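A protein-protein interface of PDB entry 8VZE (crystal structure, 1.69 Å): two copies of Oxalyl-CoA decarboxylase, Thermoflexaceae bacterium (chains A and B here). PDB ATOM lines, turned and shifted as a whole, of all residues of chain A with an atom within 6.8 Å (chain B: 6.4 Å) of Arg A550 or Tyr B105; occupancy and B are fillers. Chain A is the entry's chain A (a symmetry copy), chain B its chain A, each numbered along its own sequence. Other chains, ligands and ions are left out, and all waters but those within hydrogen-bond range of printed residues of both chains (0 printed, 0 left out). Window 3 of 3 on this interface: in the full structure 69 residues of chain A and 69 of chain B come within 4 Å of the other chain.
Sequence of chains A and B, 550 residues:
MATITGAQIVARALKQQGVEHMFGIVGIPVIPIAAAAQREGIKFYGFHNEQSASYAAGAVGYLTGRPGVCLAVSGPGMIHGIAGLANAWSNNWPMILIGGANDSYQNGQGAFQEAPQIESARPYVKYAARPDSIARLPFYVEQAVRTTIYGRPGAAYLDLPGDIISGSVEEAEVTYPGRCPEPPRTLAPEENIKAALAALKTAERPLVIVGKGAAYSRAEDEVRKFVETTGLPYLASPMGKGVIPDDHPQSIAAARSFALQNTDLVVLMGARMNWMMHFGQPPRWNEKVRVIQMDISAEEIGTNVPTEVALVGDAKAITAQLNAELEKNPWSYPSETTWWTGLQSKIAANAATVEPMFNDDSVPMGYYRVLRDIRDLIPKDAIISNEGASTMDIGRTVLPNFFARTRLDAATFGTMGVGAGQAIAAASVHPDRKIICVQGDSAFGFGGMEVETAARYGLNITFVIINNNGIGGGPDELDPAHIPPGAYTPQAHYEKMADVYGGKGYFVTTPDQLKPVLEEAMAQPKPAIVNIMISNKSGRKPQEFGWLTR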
ATOM      1  N   PHE A 279      26.305 -22.464 -17.036  1.00  0.00           N
ATOM      2  CA  PHE A 279      26.097 -22.401 -15.595  1.00  0.00           C
ATOM      3  C   PHE A 279      25.407 -23.631 -15.023  1.00  0.00           C
ATOM      4  O   PHE A 279      24.961 -23.593 -13.870  1.00  0.00           O
ATOM      5  CB  PHE A 279      25.307 -21.150 -15.221  1.00  0.00           C
ATOM      6  CG  PHE A 279      25.871 -19.886 -15.820  1.00  0.00           C
ATOM      7  CD1 PHE A 279      27.157 -19.451 -15.496  1.00  0.00           C
ATOM      8  CD2 PHE A 279      25.134 -19.153 -16.734  1.00  0.00           C
ATOM      9  CE1 PHE A 279      27.660 -18.266 -16.041  1.00  0.00           C
ATOM     10  CE2 PHE A 279      25.629 -17.965 -17.306  1.00  0.00           C
ATOM     11  CZ  PHE A 279      26.893 -17.512 -16.968  1.00  0.00           C
ATOM     12  N   GLY A 546      22.083 -20.328 -28.856  1.00  0.00           N
ATOM     13  CA  GLY A 546      23.386 -19.721 -29.009  1.00  0.00           C
ATOM     14  C   GLY A 546      24.296 -20.012 -27.827  1.00  0.00           C
ATOM     15  O   GLY A 546      23.839 -20.303 -26.722  1.00  0.00           O
ATOM     16  N   LEU A 548      26.203 -18.135 -26.060  1.00  0.00           N
ATOM     17  CA  LEU A 548      26.252 -17.137 -24.996  1.00  0.00           C
ATOM     18  C   LEU A 548      24.903 -17.151 -24.298  1.00  0.00           C
ATOM     19  O   LEU A 548      23.948 -16.515 -24.748  1.00  0.00           O
ATOM     20  CB  LEU A 548      26.586 -15.754 -25.556  1.00  0.00           C
ATOM     21  CG  LEU A 548      26.684 -14.628 -24.514  1.00  0.00           C
ATOM     22  CD1 LEU A 548      27.988 -14.727 -23.716  1.00  0.00           C
ATOM     23  CD2 LEU A 548      26.530 -13.247 -25.158  1.00  0.00           C
ATOM     24  N   THR A 549      24.819 -17.904 -23.205  1.00  0.00           N
ATOM     25  CA  THR A 549      23.599 -17.955 -22.420  1.00  0.00           C
ATOM     26  C   THR A 549      23.427 -16.637 -21.673  1.00  0.00           C
ATOM     27  O   THR A 549      24.355 -16.164 -21.008  1.00  0.00           O
ATOM     28  CB  THR A 549      23.654 -19.138 -21.446  1.00  0.00           C
ATOM     29  OG1 THR A 549      24.083 -20.305 -22.160  1.00  0.00           O
ATOM     30  CG2 THR A 549      22.286 -19.397 -20.813  1.00  0.00           C
ATOM     31  N   ARG A 550      22.257 -16.025 -21.822  1.00  0.00           N
ATOM     32  CA  ARG A 550      21.935 -14.796 -21.098  1.00  0.00           C
ATOM     33  C   ARG A 550      20.433 -14.551 -21.094  1.00  0.00           C
ATOM     34  O   ARG A 550      19.904 -13.884 -20.202  1.00  0.00           O
ATOM     35  CB  ARG A 550      22.675 -13.592 -21.701  1.00  0.00           C
ATOM     36  CG  ARG A 550      22.439 -13.362 -23.194  1.00  0.00           C
ATOM     37  CD  ARG A 550      23.255 -12.172 -23.725  1.00  0.00           C
ATOM     38  NE  ARG A 550      23.117 -10.955 -22.923  1.00  0.00           N
ATOM     39  CZ  ARG A 550      22.349  -9.920 -23.243  1.00  0.00           C
ATOM     40  NH1 ARG A 550      21.617  -9.916 -24.347  1.00  0.00           N
ATOM     41  NH2 ARG A 550      22.315  -8.858 -22.433  1.00  0.00           N
ATOM     42  N   ASN B 102      30.119  -8.156 -17.952  1.00  0.00           N
ATOM     43  CA  ASN B 102      29.104  -9.191 -18.098  1.00  0.00           C
ATOM     44  C   ASN B 102      27.768  -8.693 -17.541  1.00  0.00           C
ATOM     45  O   ASN B 102      27.710  -7.728 -16.776  1.00  0.00           O
ATOM     46  CB  ASN B 102      29.564 -10.473 -17.398  1.00  0.00           C
ATOM     47  CG  ASN B 102      29.758 -10.280 -15.923  1.00  0.00           C
ATOM     48  OD1 ASN B 102      30.836  -9.905 -15.457  1.00  0.00           O
ATOM     49  ND2 ASN B 102      28.689 -10.501 -15.167  1.00  0.00           N
ATOM     50  N   ASP B 103      26.678  -9.326 -17.983  1.00  0.00           N
ATOM     51  CA  ASP B 103      25.348  -8.959 -17.495  1.00  0.00           C
ATOM     52  C   ASP B 103      25.315  -9.038 -15.982  1.00  0.00           C
ATOM     53  O   ASP B 103      25.793 -10.011 -15.403  1.00  0.00           O
ATOM     54  CB  ASP B 103      24.289  -9.922 -18.032  1.00  0.00           C
ATOM     55  CG  ASP B 103      24.049  -9.779 -19.517  1.00  0.00           C
ATOM     56  OD1 ASP B 103      24.250  -8.679 -20.052  1.00  0.00           O
ATOM     57  OD2 ASP B 103      23.644 -10.786 -20.145  1.00  0.00           O
ATOM     58  N   SER B 104      24.710  -8.030 -15.344  1.00  0.00           N
ATOM     59  CA  SER B 104      24.815  -7.910 -13.893  1.00  0.00           C
ATOM     60  C   SER B 104      24.196  -9.106 -13.181  1.00  0.00           C
ATOM     61  O   SER B 104      24.669  -9.501 -12.097  1.00  0.00           O
ATOM     62  CB  SER B 104      24.141  -6.604 -13.427  1.00  0.00           C
ATOM     63  OG  SER B 104      22.757  -6.632 -13.757  1.00  0.00           O
ATOM     64  N   TYR B 105      23.141  -9.694 -13.755  1.00  0.00           N
ATOM     65  CA  TYR B 105      22.473 -10.805 -13.096  1.00  0.00           C
ATOM     66  C   TYR B 105      23.225 -12.121 -13.244  1.00  0.00           C
ATOM     67  O   TYR B 105      22.739 -13.139 -12.751  1.00  0.00           O
ATOM     68  CB  TYR B 105      21.029 -10.960 -13.616  1.00  0.00           C
ATOM     69  CG  TYR B 105      20.957 -11.040 -15.128  1.00  0.00           C
ATOM     70  CD1 TYR B 105      21.149 -12.253 -15.793  1.00  0.00           C
ATOM     71  CD2 TYR B 105      20.724  -9.893 -15.891  1.00  0.00           C
ATOM     72  CE1 TYR B 105      21.101 -12.325 -17.188  1.00  0.00           C
ATOM     73  CE2 TYR B 105      20.664  -9.964 -17.276  1.00  0.00           C
ATOM     74  CZ  TYR B 105      20.856 -11.170 -17.910  1.00  0.00           C
ATOM     75  OH  TYR B 105      20.808 -11.191 -19.283  1.00  0.00           O
ATOM     76  N   GLN B 106      24.411 -12.110 -13.874  1.00  0.00           N
ATOM     77  CA  GLN B 106      25.300 -13.267 -13.898  1.00  0.00           C
ATOM     78  C   GLN B 106      26.519 -13.082 -13.006  1.00  0.00           C
ATOM     79  O   GLN B 106      27.397 -13.957 -12.991  1.00  0.00           O
ATOM     80  CB  GLN B 106      25.757 -13.557 -15.326  1.00  0.00           C
ATOM     81  CG  GLN B 106      24.581 -13.965 -16.188  1.00  0.00           C
ATOM     82  CD  GLN B 106      24.966 -14.164 -17.634  1.00  0.00           C
ATOM     83  OE1 GLN B 106      26.007 -13.683 -18.081  1.00  0.00           O
ATOM     84  NE2 GLN B 106      24.121 -14.868 -18.375  1.00  0.00           N
ATOM     85  N   ASN B 107      26.606 -11.976 -12.269  1.00  0.00           N
ATOM     86  CA  ASN B 107      27.731 -11.806 -11.353  1.00  0.00           C
ATOM     87  C   ASN B 107      27.794 -12.981 -10.372  1.00  0.00           C
ATOM     88  O   ASN B 107      26.774 -13.444  -9.853  1.00  0.00           O
ATOM     89  CB  ASN B 107      27.611 -10.496 -10.575  1.00  0.00           C
ATOM     90  CG  ASN B 107      28.033  -9.266 -11.384  1.00  0.00           C
ATOM     91  OD1 ASN B 107      28.439  -9.369 -12.538  1.00  0.00           O
ATOM     92  ND2 ASN B 107      27.974  -8.088 -10.752  1.00  0.00           N
ATOM     93  N   GLN B 109      28.687 -15.969 -11.113  1.00  0.00           N
ATOM     94  CA  GLN B 109      28.451 -17.265 -11.728  1.00  0.00           C
ATOM     95  C   GLN B 109      29.626 -17.765 -12.554  1.00  0.00           C
ATOM     96  O   GLN B 109      29.558 -18.892 -13.058  1.00  0.00           O
ATOM     97  CB  GLN B 109      27.219 -17.208 -12.645  1.00  0.00           C
ATOM     98  CG  GLN B 109      25.957 -16.690 -11.968  1.00  0.00           C
ATOM     99  CD  GLN B 109      24.743 -17.123 -12.736  1.00  0.00           C
ATOM    100  OE1 GLN B 109      24.338 -16.474 -13.687  1.00  0.00           O
ATOM    101  NE2 GLN B 109      24.192 -18.267 -12.370  1.00  0.00           N
ATOM    102  N   GLY B 162      26.484  -5.540 -19.608  1.00  0.00           N
ATOM    103  CA  GLY B 162      25.822  -5.755 -20.879  1.00  0.00           C
ATOM    104  C   GLY B 162      24.330  -5.479 -20.837  1.00  0.00           C
ATOM    105  O   GLY B 162      23.747  -5.069 -21.844  1.00  0.00           O
ATOM    106  N   ASP B 163      23.687  -5.705 -19.682  1.00  0.00           N
ATOM    107  CA  ASP B 163      22.245  -5.480 -19.612  1.00  0.00           C
ATOM    108  C   ASP B 163      21.882  -4.007 -19.490  1.00  0.00           C
ATOM    109  O   ASP B 163      20.754  -3.639 -19.842  1.00  0.00           O
ATOM    110  CB  ASP B 163      21.605  -6.288 -18.470  1.00  0.00           C
ATOM    111  CG  ASP B 163      22.320  -6.138 -17.132  1.00  0.00           C
ATOM    112  OD1 ASP B 163      23.565  -5.978 -17.086  1.00  0.00           O
ATOM    113  OD2 ASP B 163      21.612  -6.223 -16.103  1.00  0.00           O
ATOM    114  N   SER B 166      22.143  -3.123 -23.391  1.00  0.00           N
ATOM    115  CA  SER B 166      21.132  -3.650 -24.302  1.00  0.00           C
ATOM    116  C   SER B 166      19.707  -3.402 -23.825  1.00  0.00           C
ATOM    117  O   SER B 166      18.772  -3.499 -24.635  1.00  0.00           O
ATOM    118  CB  SER B 166      21.343  -5.150 -24.489  1.00  0.00           C
ATOM    119  OG  SER B 166      21.093  -5.782 -23.254  1.00  0.00           O
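Of the 10 printed residues of chain B, 5 touch a printed residue of chain A.
Hydrophobic or aromatic side chains of chain B that line the printed part of chain A: Tyr B105.
Printed residues of chain A that touch a printed residue of chain B: Phe A279, Thr A549 and Arg A550.
Hydrophobic or aromatic side chains of chain A that line the printed part of chain B: Phe A279.
Among the printed residues, 7 pairs touch across the chains.
Phe A279 touches Gln B106.
O of Gln B109 touches CD1 of Phe A279, 3.5 Å away.
Gln B106 touches Arg A550.
No position is printed for both chains.
Of the 7 pairs that touch across the chains among the printed residues, none has its exchanged pair printed and touching as well.
The side-chain carboxylate (OD2) of Asp B103 lies within hydrogen-bond range of the side-chain hydroxyl (OH) of Tyr B105 (3.0 Å).
OD1 of Asp B103 sits at hydrogen-bond distance from N of Asp B163.
O of Gly B162 sits at hydrogen-bond distance from OG of Ser B166, 3.1 Å away.
The guanidinium group (NE) of Arg A550 is in salt-bridge range of the side-chain carboxylate (OD2) of Asp B103.
The side-chain hydroxyl (OH) of Tyr B105 lies within hydrogen-bond range of the backbone carbonyl oxygen (O) of Arg A550 (3.0 Å).
O of Thr A549 sits at hydrogen-bond distance from NE2 of Gln B106 (2.9 Å).
The guanidinium group (NH2) of Arg A550 lies within hydrogen-bond range of the side-chain hydroxyl (OG) of Ser B166 (3.4 Å).
Arg A550 touches four residues of chain B.
Of chain A, only Arg A550 (3.0 Å) comes within 4 Å of Tyr B105.
Of the printed residues of chain B, Phe A279 touches Gln B106 and Gln B109.
Printed residues of chain B within 4 Å of Thr A549: Gln B106 (2.9 Å).
Of the printed residues of chain A, Asp B103 touches Arg A550.
Of the printed residues of chain A, Gln B109 touches Phe A279.
Of the printed residues of chain A, Gln B106 touches Phe A279 (3.6 Å), Thr A549 (2.9 Å) and Arg A550 (3.5 Å).
The nearest residue of chain B that does not touch Arg A550 is Gly B162 (4.1 Å).
The nearest printed residue of chain A that does not touch Asp B103 is Thr A549 (5.5 Å).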
